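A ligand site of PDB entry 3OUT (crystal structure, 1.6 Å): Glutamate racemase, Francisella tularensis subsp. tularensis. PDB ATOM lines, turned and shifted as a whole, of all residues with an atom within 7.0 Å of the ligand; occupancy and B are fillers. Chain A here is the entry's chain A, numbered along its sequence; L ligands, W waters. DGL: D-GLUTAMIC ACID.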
ATOM      1  N   ASP A  14     -11.210 -15.735  10.888  1.00  0.00           N
ATOM      2  CA  ASP A  14     -10.384 -16.739  10.254  1.00  0.00           C
ATOM      3  C   ASP A  14     -11.038 -17.275   8.970  1.00  0.00           C
ATOM      4  O   ASP A  14     -12.212 -17.151   8.789  1.00  0.00           O
ATOM      5  CB  ASP A  14     -10.215 -17.924  11.212  1.00  0.00           C
ATOM      6  CG  ASP A  14      -9.030 -18.865  10.878  1.00  0.00           C
ATOM      7  OD1 ASP A  14      -8.237 -18.582  10.040  1.00  0.00           O
ATOM      8  OD2 ASP A  14      -8.959 -19.886  11.547  1.00  0.00           O
ATOM      9  N   SER A  15     -10.223 -17.882   8.132  1.00  0.00           N
ATOM     10  CA  SER A  15     -10.703 -18.759   7.101  1.00  0.00           C
ATOM     11  C   SER A  15     -11.156 -20.077   7.784  1.00  0.00           C
ATOM     12  O   SER A  15     -12.242 -20.475   7.732  1.00  0.00           O
ATOM     13  CB  SER A  15      -9.620 -19.021   6.065  1.00  0.00           C
ATOM     14  OG  SER A  15      -8.383 -19.264   6.623  1.00  0.00           O
ATOM     15  N   GLY A  16     -10.243 -20.682   8.505  1.00  0.00           N
ATOM     16  CA  GLY A  16     -10.591 -21.771   9.364  1.00  0.00           C
ATOM     17  C   GLY A  16      -9.436 -22.529   9.937  1.00  0.00           C
ATOM     18  O   GLY A  16      -8.359 -22.642   9.292  1.00  0.00           O
ATOM     19  N   ILE A  17      -9.619 -23.017  11.174  1.00  0.00           N
ATOM     20  CA  ILE A  17      -8.676 -23.885  11.877  1.00  0.00           C
ATOM     21  C   ILE A  17      -7.395 -23.265  12.402  1.00  0.00           C
ATOM     22  O   ILE A  17      -7.139 -23.323  13.593  1.00  0.00           O
ATOM     23  CB  ILE A  17      -8.290 -25.157  11.109  1.00  0.00           C
ATOM     24  CG1 ILE A  17      -9.559 -25.944  10.795  1.00  0.00           C
ATOM     25  CG2 ILE A  17      -7.297 -25.982  11.964  1.00  0.00           C
ATOM     26  CD1 ILE A  17      -9.379 -27.149   9.862  1.00  0.00           C
ATOM     27  N   GLY A  18      -6.582 -22.652  11.547  1.00  0.00           N
ATOM     28  CA  GLY A  18      -5.284 -22.135  12.046  1.00  0.00           C
ATOM     29  C   GLY A  18      -5.324 -20.862  12.859  1.00  0.00           C
ATOM     30  O   GLY A  18      -4.425 -20.558  13.656  1.00  0.00           O
ATOM     31  N   GLY A  19      -6.388 -20.089  12.680  1.00  0.00           N
ATOM     32  CA  GLY A  19      -6.592 -18.824  13.391  1.00  0.00           C
ATOM     33  C   GLY A  19      -6.916 -19.044  14.869  1.00  0.00           C
ATOM     34  O   GLY A  19      -6.964 -18.092  15.659  1.00  0.00           O
ATOM     35  N   ARG A  43     -16.016 -24.064   3.715  1.00  0.00           N
ATOM     36  CA  ARG A  43     -15.441 -23.650   2.437  1.00  0.00           C
ATOM     37  C   ARG A  43     -13.928 -23.589   2.410  1.00  0.00           C
ATOM     38  O   ARG A  43     -13.378 -23.302   1.389  1.00  0.00           O
ATOM     39  CB  ARG A  43     -16.082 -22.328   1.987  1.00  0.00           C
ATOM     40  CG  ARG A  43     -17.601 -22.431   1.909  1.00  0.00           C
ATOM     41  CD  ARG A  43     -18.198 -21.192   1.279  1.00  0.00           C
ATOM     42  NE  ARG A  43     -18.009 -19.992   2.081  1.00  0.00           N
ATOM     43  CZ  ARG A  43     -18.745 -18.868   2.033  1.00  0.00           C
ATOM     44  NH1 ARG A  43     -19.772 -18.738   1.171  1.00  0.00           N
ATOM     45  NH2 ARG A  43     -18.416 -17.830   2.811  1.00  0.00           N
ATOM     46  N   ILE A  44     -13.272 -23.872   3.528  1.00  0.00           N
ATOM     47  CA  ILE A  44     -11.814 -24.016   3.498  1.00  0.00           C
ATOM     48  C   ILE A  44     -11.348 -25.187   2.612  1.00  0.00           C
ATOM     49  O   ILE A  44     -12.044 -26.183   2.399  1.00  0.00           O
ATOM     50  CB  ILE A  44     -11.204 -24.129   4.931  1.00  0.00           C
ATOM     51  CG1 ILE A  44     -11.787 -25.320   5.702  1.00  0.00           C
ATOM     52  CG2 ILE A  44     -11.298 -22.754   5.664  1.00  0.00           C
ATOM     53  CD1 ILE A  44     -11.050 -25.650   7.062  1.00  0.00           C
ATOM     54  N   PRO A  45     -10.129 -25.069   2.069  1.00  0.00           N
ATOM     55  CA  PRO A  45      -9.188 -23.981   2.249  1.00  0.00           C
ATOM     56  C   PRO A  45      -9.477 -22.769   1.411  1.00  0.00           C
ATOM     57  O   PRO A  45     -10.051 -22.897   0.303  1.00  0.00           O
ATOM     58  CB  PRO A  45      -7.858 -24.597   1.786  1.00  0.00           C
ATOM     59  CG  PRO A  45      -8.252 -25.541   0.713  1.00  0.00           C
ATOM     60  CD  PRO A  45      -9.571 -26.112   1.183  1.00  0.00           C
ATOM     61  N   TYR A  46      -9.046 -21.606   1.900  1.00  0.00           N
ATOM     62  CA  TYR A  46      -9.012 -20.377   1.093  1.00  0.00           C
ATOM     63  C   TYR A  46      -7.722 -20.238   0.264  1.00  0.00           C
ATOM     64  O   TYR A  46      -7.689 -19.519  -0.734  1.00  0.00           O
ATOM     65  CB  TYR A  46      -9.140 -19.146   1.983  1.00  0.00           C
ATOM     66  CG  TYR A  46     -10.519 -18.790   2.535  1.00  0.00           C
ATOM     67  CD1 TYR A  46     -11.506 -19.756   2.761  1.00  0.00           C
ATOM     68  CD2 TYR A  46     -10.802 -17.486   2.903  1.00  0.00           C
ATOM     69  CE1 TYR A  46     -12.712 -19.416   3.326  1.00  0.00           C
ATOM     70  CE2 TYR A  46     -12.024 -17.122   3.422  1.00  0.00           C
ATOM     71  CZ  TYR A  46     -12.998 -18.116   3.613  1.00  0.00           C
ATOM     72  OH  TYR A  46     -14.181 -17.749   4.163  1.00  0.00           O
ATOM     73  N   GLY A  47      -6.664 -20.917   0.718  1.00  0.00           N
ATOM     74  CA  GLY A  47      -5.316 -20.623   0.228  1.00  0.00           C
ATOM     75  C   GLY A  47      -5.047 -21.039  -1.195  1.00  0.00           C
ATOM     76  O   GLY A  47      -4.041 -20.631  -1.789  1.00  0.00           O
ATOM     77  N   THR A  48      -5.924 -21.887  -1.740  1.00  0.00           N
ATOM     78  CA  THR A  48      -5.818 -22.280  -3.140  1.00  0.00           C
ATOM     79  C   THR A  48      -6.967 -21.734  -4.016  1.00  0.00           C
ATOM     80  O   THR A  48      -7.105 -22.141  -5.170  1.00  0.00           O
ATOM     81  CB  THR A  48      -5.783 -23.793  -3.235  1.00  0.00           C
ATOM     82  OG1 THR A  48      -6.919 -24.323  -2.540  1.00  0.00           O
ATOM     83  CG2 THR A  48      -4.530 -24.332  -2.573  1.00  0.00           C
ATOM     84  N   ALA A  76      -6.978 -13.201  11.584  1.00  0.00           N
ATOM     85  CA  ALA A  76      -5.997 -14.175  11.944  1.00  0.00           C
ATOM     86  C   ALA A  76      -5.358 -14.876  10.757  1.00  0.00           C
ATOM     87  O   ALA A  76      -4.219 -15.357  10.874  1.00  0.00           O
ATOM     88  CB  ALA A  76      -6.650 -15.231  12.913  1.00  0.00           C
ATOM     89  N   CYS A  77      -6.036 -14.853   9.596  1.00  0.00           N
ATOM     90  CA  CYS A  77      -5.626 -15.593   8.403  1.00  0.00           C
ATOM     91  C   CYS A  77      -4.812 -14.684   7.482  1.00  0.00           C
ATOM     92  O   CYS A  77      -5.222 -13.577   7.178  1.00  0.00           O
ATOM     93  CB  CYS A  77      -6.878 -16.089   7.675  1.00  0.00           C
ATOM     94  SG  CYS A  77      -6.636 -16.817   6.077  1.00  0.00           S
ATOM     95  N   ASN A  78      -3.635 -15.148   7.081  1.00  0.00           N
ATOM     96  CA  ASN A  78      -2.773 -14.412   6.166  1.00  0.00           C
ATOM     97  C   ASN A  78      -3.414 -14.277   4.792  1.00  0.00           C
ATOM     98  O   ASN A  78      -3.237 -13.267   4.129  1.00  0.00           O
ATOM     99  CB  ASN A  78      -1.415 -15.088   6.029  1.00  0.00           C
ATOM    100  CG  ASN A  78      -0.560 -15.014   7.286  1.00  0.00           C
ATOM    101  OD1 ASN A  78       0.336 -14.141   7.377  1.00  0.00           O
ATOM    102  ND2 ASN A  78      -0.779 -15.928   8.235  1.00  0.00           N
ATOM    103  N   THR A  79      -4.144 -15.300   4.392  1.00  0.00           N
ATOM    104  CA  THR A  79      -4.780 -15.305   3.063  1.00  0.00           C
ATOM    105  C   THR A  79      -5.867 -14.198   2.976  1.00  0.00           C
ATOM    106  O   THR A  79      -5.868 -13.396   2.023  1.00  0.00           O
ATOM    107  CB  THR A  79      -5.301 -16.736   2.694  1.00  0.00           C
ATOM    108  OG1 THR A  79      -4.211 -17.710   2.664  1.00  0.00           O
ATOM    109  CG2 THR A  79      -5.933 -16.697   1.329  1.00  0.00           C
ATOM    110  N   ILE A  80      -6.783 -14.145   3.945  1.00  0.00           N
ATOM    111  CA  ILE A  80      -7.769 -13.050   3.970  1.00  0.00           C
ATOM    112  C   ILE A  80      -7.081 -11.699   4.112  1.00  0.00           C
ATOM    113  O   ILE A  80      -7.494 -10.707   3.496  1.00  0.00           O
ATOM    114  CB  ILE A  80      -8.770 -13.288   5.134  1.00  0.00           C
ATOM    115  CG1 ILE A  80      -9.544 -14.581   4.902  1.00  0.00           C
ATOM    116  CG2 ILE A  80      -9.705 -12.136   5.314  1.00  0.00           C
ATOM    117  CD1 ILE A  80     -10.447 -14.986   6.087  1.00  0.00           C
ATOM    118  N   VAL A 100      -2.723  -9.975  10.487  1.00  0.00           N
ATOM    119  CA  VAL A 100      -1.462 -10.682  10.742  1.00  0.00           C
ATOM    120  C   VAL A 100      -0.325 -10.257   9.791  1.00  0.00           C
ATOM    121  O   VAL A 100       0.871 -10.352  10.150  1.00  0.00           O
ATOM    122  CB  VAL A 100      -1.601 -12.226  10.724  1.00  0.00           C
ATOM    123  CG1 VAL A 100      -2.259 -12.724  11.995  1.00  0.00           C
ATOM    124  CG2 VAL A 100      -2.320 -12.764   9.468  1.00  0.00           C
ATOM    125  N   ALA A 118       4.054 -18.811   2.286  1.00  0.00           N
ATOM    126  CA  ALA A 118       2.633 -18.615   2.524  1.00  0.00           C
ATOM    127  C   ALA A 118       1.852 -19.532   1.575  1.00  0.00           C
ATOM    128  O   ALA A 118       2.424 -20.276   0.748  1.00  0.00           O
ATOM    129  CB  ALA A 118       2.241 -17.174   2.292  1.00  0.00           C
ATOM    130  N   THR A 119       0.516 -19.448   1.645  1.00  0.00           N
ATOM    131  CA  THR A 119      -0.320 -20.157   0.692  1.00  0.00           C
ATOM    132  C   THR A 119      -0.114 -19.679  -0.734  1.00  0.00           C
ATOM    133  O   THR A 119       0.272 -18.560  -0.969  1.00  0.00           O
ATOM    134  CB  THR A 119      -1.811 -19.988   1.010  1.00  0.00           C
ATOM    135  OG1 THR A 119      -2.204 -18.620   0.913  1.00  0.00           O
ATOM    136  CG2 THR A 119      -2.167 -20.602   2.392  1.00  0.00           C
ATOM    137  N   THR A 122      -1.758 -16.240  -1.098  1.00  0.00           N
ATOM    138  CA  THR A 122      -1.057 -15.163  -0.412  1.00  0.00           C
ATOM    139  C   THR A 122       0.175 -14.770  -1.222  1.00  0.00           C
ATOM    140  O   THR A 122       0.378 -13.583  -1.450  1.00  0.00           O
ATOM    141  CB  THR A 122      -0.665 -15.560   0.977  1.00  0.00           C
ATOM    142  OG1 THR A 122      -1.865 -15.731   1.738  1.00  0.00           O
ATOM    143  CG2 THR A 122       0.184 -14.469   1.702  1.00  0.00           C
ATOM    144  N   VAL A 150      -0.729 -26.771   4.259  1.00  0.00           N
ATOM    145  CA  VAL A 150      -2.006 -26.638   5.000  1.00  0.00           C
ATOM    146  C   VAL A 150      -2.691 -28.009   5.162  1.00  0.00           C
ATOM    147  O   VAL A 150      -2.954 -28.437   6.301  1.00  0.00           O
ATOM    148  CB  VAL A 150      -2.932 -25.569   4.411  1.00  0.00           C
ATOM    149  CG1 VAL A 150      -4.392 -25.744   4.961  1.00  0.00           C
ATOM    150  CG2 VAL A 150      -2.439 -24.150   4.768  1.00  0.00           C
ATOM    151  N   GLU A 154      -3.162 -30.355   8.545  1.00  0.00           N
ATOM    152  CA  GLU A 154      -4.526 -30.682   9.015  1.00  0.00           C
ATOM    153  C   GLU A 154      -4.759 -32.210   9.032  1.00  0.00           C
ATOM    154  O   GLU A 154      -5.627 -32.707   9.773  1.00  0.00           O
ATOM    155  CB  GLU A 154      -5.588 -29.907   8.210  1.00  0.00           C
ATOM    156  CG  GLU A 154      -5.621 -28.443   8.500  1.00  0.00           C
ATOM    157  CD  GLU A 154      -6.662 -27.653   7.728  1.00  0.00           C
ATOM    158  OE1 GLU A 154      -7.449 -28.315   6.978  1.00  0.00           O
ATOM    159  OE2 GLU A 154      -6.740 -26.422   7.913  1.00  0.00           O
ATOM    160  N   LEU A 184       6.831 -16.928   8.525  1.00  0.00           N
ATOM    161  CA  LEU A 184       5.893 -18.040   8.457  1.00  0.00           C
ATOM    162  C   LEU A 184       4.537 -17.396   8.203  1.00  0.00           C
ATOM    163  O   LEU A 184       3.737 -17.185   9.133  1.00  0.00           O
ATOM    164  CB  LEU A 184       5.919 -18.837   9.737  1.00  0.00           C
ATOM    165  CG  LEU A 184       7.281 -19.429  10.123  1.00  0.00           C
ATOM    166  CD1 LEU A 184       7.188 -20.269  11.404  1.00  0.00           C
ATOM    167  CD2 LEU A 184       7.912 -20.236   8.992  1.00  0.00           C
ATOM    168  N   GLY A 185       4.277 -17.076   6.934  1.00  0.00           N
ATOM    169  CA  GLY A 185       3.134 -16.297   6.504  1.00  0.00           C
ATOM    170  C   GLY A 185       1.841 -17.083   6.248  1.00  0.00           C
ATOM    171  O   GLY A 185       1.065 -16.738   5.387  1.00  0.00           O
ATOM    172  N   CYS A 186       1.635 -18.085   7.071  1.00  0.00           N
ATOM    173  CA  CYS A 186       0.409 -18.895   7.116  1.00  0.00           C
ATOM    174  C   CYS A 186       0.256 -19.398   8.537  1.00  0.00           C
ATOM    175  O   CYS A 186       1.231 -19.889   9.142  1.00  0.00           O
ATOM    176  CB  CYS A 186       0.548 -20.075   6.158  1.00  0.00           C
ATOM    177  SG  CYS A 186      -0.857 -21.255   6.167  1.00  0.00           S
ATOM    178  N   THR A 187      -0.965 -19.344   9.083  1.00  0.00           N
ATOM    179  CA  THR A 187      -1.224 -19.777  10.455  1.00  0.00           C
ATOM    180  C   THR A 187      -0.715 -21.172  10.775  1.00  0.00           C
ATOM    181  O   THR A 187      -0.373 -21.451  11.937  1.00  0.00           O
ATOM    182  CB  THR A 187      -2.758 -19.810  10.755  1.00  0.00           C
ATOM    183  OG1 THR A 187      -3.388 -20.542   9.723  1.00  0.00           O
ATOM    184  CG2 THR A 187      -3.383 -18.408  10.823  1.00  0.00           C
ATOM    185  N   HIS A 188      -0.721 -22.065   9.792  1.00  0.00           N
ATOM    186  CA  HIS A 188      -0.399 -23.466   9.993  1.00  0.00           C
ATOM    187  C   HIS A 188       1.099 -23.731  10.168  1.00  0.00           C
ATOM    188  O   HIS A 188       1.468 -24.746  10.745  1.00  0.00           O
ATOM    189  CB  HIS A 188      -0.935 -24.308   8.852  1.00  0.00           C
ATOM    190  CG  HIS A 188      -2.427 -24.422   8.830  1.00  0.00           C
ATOM    191  ND1 HIS A 188      -3.264 -23.342   8.926  1.00  0.00           N
ATOM    192  CD2 HIS A 188      -3.229 -25.499   8.631  1.00  0.00           C
ATOM    193  CE1 HIS A 188      -4.520 -23.751   8.817  1.00  0.00           C
ATOM    194  NE2 HIS A 188      -4.522 -25.054   8.683  1.00  0.00           N
ATOM    195  N   TYR A 189       1.938 -22.865   9.626  1.00  0.00           N
ATOM    196  CA  TYR A 189       3.331 -23.239   9.438  1.00  0.00           C
ATOM    197  C   TYR A 189       4.140 -23.330  10.746  1.00  0.00           C
ATOM    198  O   TYR A 189       5.024 -24.163  10.825  1.00  0.00           O
ATOM    199  CB  TYR A 189       4.034 -22.364   8.410  1.00  0.00           C
ATOM    200  CG  TYR A 189       3.434 -22.356   6.997  1.00  0.00           C
ATOM    201  CD1 TYR A 189       2.414 -23.242   6.630  1.00  0.00           C
ATOM    202  CD2 TYR A 189       3.897 -21.464   6.036  1.00  0.00           C
ATOM    203  CE1 TYR A 189       1.844 -23.184   5.328  1.00  0.00           C
ATOM    204  CE2 TYR A 189       3.395 -21.427   4.781  1.00  0.00           C
ATOM    205  CZ  TYR A 189       2.380 -22.278   4.425  1.00  0.00           C
ATOM    206  OH  TYR A 189       1.841 -22.201   3.178  1.00  0.00           O
HETATM  207  N   DGL L   1      -6.740 -21.565   6.707  1.00  0.00           N
HETATM  208  CA  DGL L   1      -5.752 -21.561   5.588  1.00  0.00           C
HETATM  209  C   DGL L   1      -6.517 -21.840   4.298  1.00  0.00           C
HETATM  210  O   DGL L   1      -7.765 -21.695   4.270  1.00  0.00           O
HETATM  211  CB  DGL L   1      -5.018 -20.244   5.386  1.00  0.00           C
HETATM  212  CG  DGL L   1      -4.280 -19.742   6.648  1.00  0.00           C
HETATM  213  CD  DGL L   1      -3.323 -18.588   6.382  1.00  0.00           C
HETATM  214  OE1 DGL L   1      -3.083 -18.252   5.190  1.00  0.00           O
HETATM  215  OE2 DGL L   1      -2.848 -17.960   7.360  1.00  0.00           O
HETATM  216  OXT DGL L   1      -5.906 -22.134   3.268  1.00  0.00           O
HETATM  217  O   HOH W   1      -0.843 -17.680   3.704  1.00  0.00           O
HETATM  218  O   HOH W   2      -4.497 -23.767   1.472  1.00  0.00           O
HETATM  219  O   HOH W   3      -7.620 -24.241   6.458  1.00  0.00           O
HETATM  220  O   HOH W   4      -6.187 -20.535   9.329  1.00  0.00           O
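The side-chain sulfur of Cys 77 sits at hydrogen-bond distance from the backbone NH of Ile 80 (3.4 Å).
SG of Cys 77 is in hydrogen-bond range of OG of Ser 15 (3.1 Å).
The backbone NH (N) of Thr 119 sits at hydrogen-bond distance from the side-chain hydroxyl (OH) of Tyr 189 (3.4 Å).
OG of Ser 15 is in hydrogen-bond range of OD1 of Asp 14.
N of Thr 79 lies close to SG of Cys 77, 3.4 Å away.
The backbone NH of Gly 16 lies close to the side-chain carboxylate of Asp 14, at 3.3 Å.
The side-chain hydroxyl (OG1) of Thr 187 sits at hydrogen-bond distance from a ring nitrogen (ND1) of His 188, at 2.9 Å.
OD1 of Asn 78 sits close to O of Gly 185, at 3.4 Å.
Residues that only touch the ligand: Ile 44 (3.9 Å), Pro 45 (3.4 Å), Cys 77 (3.8 Å), Thr 119 (3.8 Å), Cys 186 (3.4 Å) and His 188 (3.8 Å).
Hydrophobic or aromatic side chains within 4 Å of the ligand: Ile 44, Pro 45, Tyr 46 and His 188.
Within 4 Å of the ligand: Ser 15, Gly 16, Ile 44, Pro 45, Tyr 46, Gly 47, Cys 77, Asn 78, Thr 79, Thr 119, Cys 186, Thr 187 and His 188.
Along chain A the residues within 4 Å of the ligand span positions 15 to 188.
The nearest printed residue that does not touch the ligand is Val 150 (4.3 Å).
N of Thr 187 sits at hydrogen-bond distance from OE2 of the ligand, 2.9 Å away.
N of Tyr 46 sits at hydrogen-bond distance from O of the ligand (2.7 Å).
The backbone NH (N) of Gly 47 is in hydrogen-bond range of an oxygen (OXT) of the ligand, 2.9 Å away.
An oxygen (OE2) of the ligand is in hydrogen-bond range of the backbone NH of Asn 78.
N of the ligand lies within hydrogen-bond range of OG of Ser 15, at 2.8 Å.
The side-chain hydroxyl (OG1) of Thr 79 lies within hydrogen-bond range of an oxygen (OE1) of the ligand (2.8 Å).
The backbone NH (N) of Thr 79 lies within hydrogen-bond range of an oxygen (OE1) of the ligand (3.2 Å).
ND2 of Asn 78 lies within hydrogen-bond range of OE2 of the ligand (3.0 Å).
O of Gly 16 sits at hydrogen-bond distance from N of the ligand, at 3.2 Å.
Water W1 lies within hydrogen-bond range of the backbone carbonyl oxygen of Gly 185 (2.7 Å), an oxygen (OE1) of the ligand (2.7 Å), the side-chain hydroxyl of Thr 122 (3.0 Å) and the backbone NH of Thr 119 (3.0 Å).
Water W3 lies within hydrogen-bond range of OE2 of Glu 154 (2.8 Å), N of the ligand (2.8 Å) and O of Gly 16 (3.3 Å).
Water W4 lies within hydrogen-bond range of the side-chain hydroxyl (OG1) of Thr 187, a nitrogen (N) of the ligand, the side-chain carboxylate (OD1) of Asp 14, the backbone carbonyl oxygen (O) of Gly 16, the backbone NH (N) of Gly 18 and the backbone NH (N) of Gly 19.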
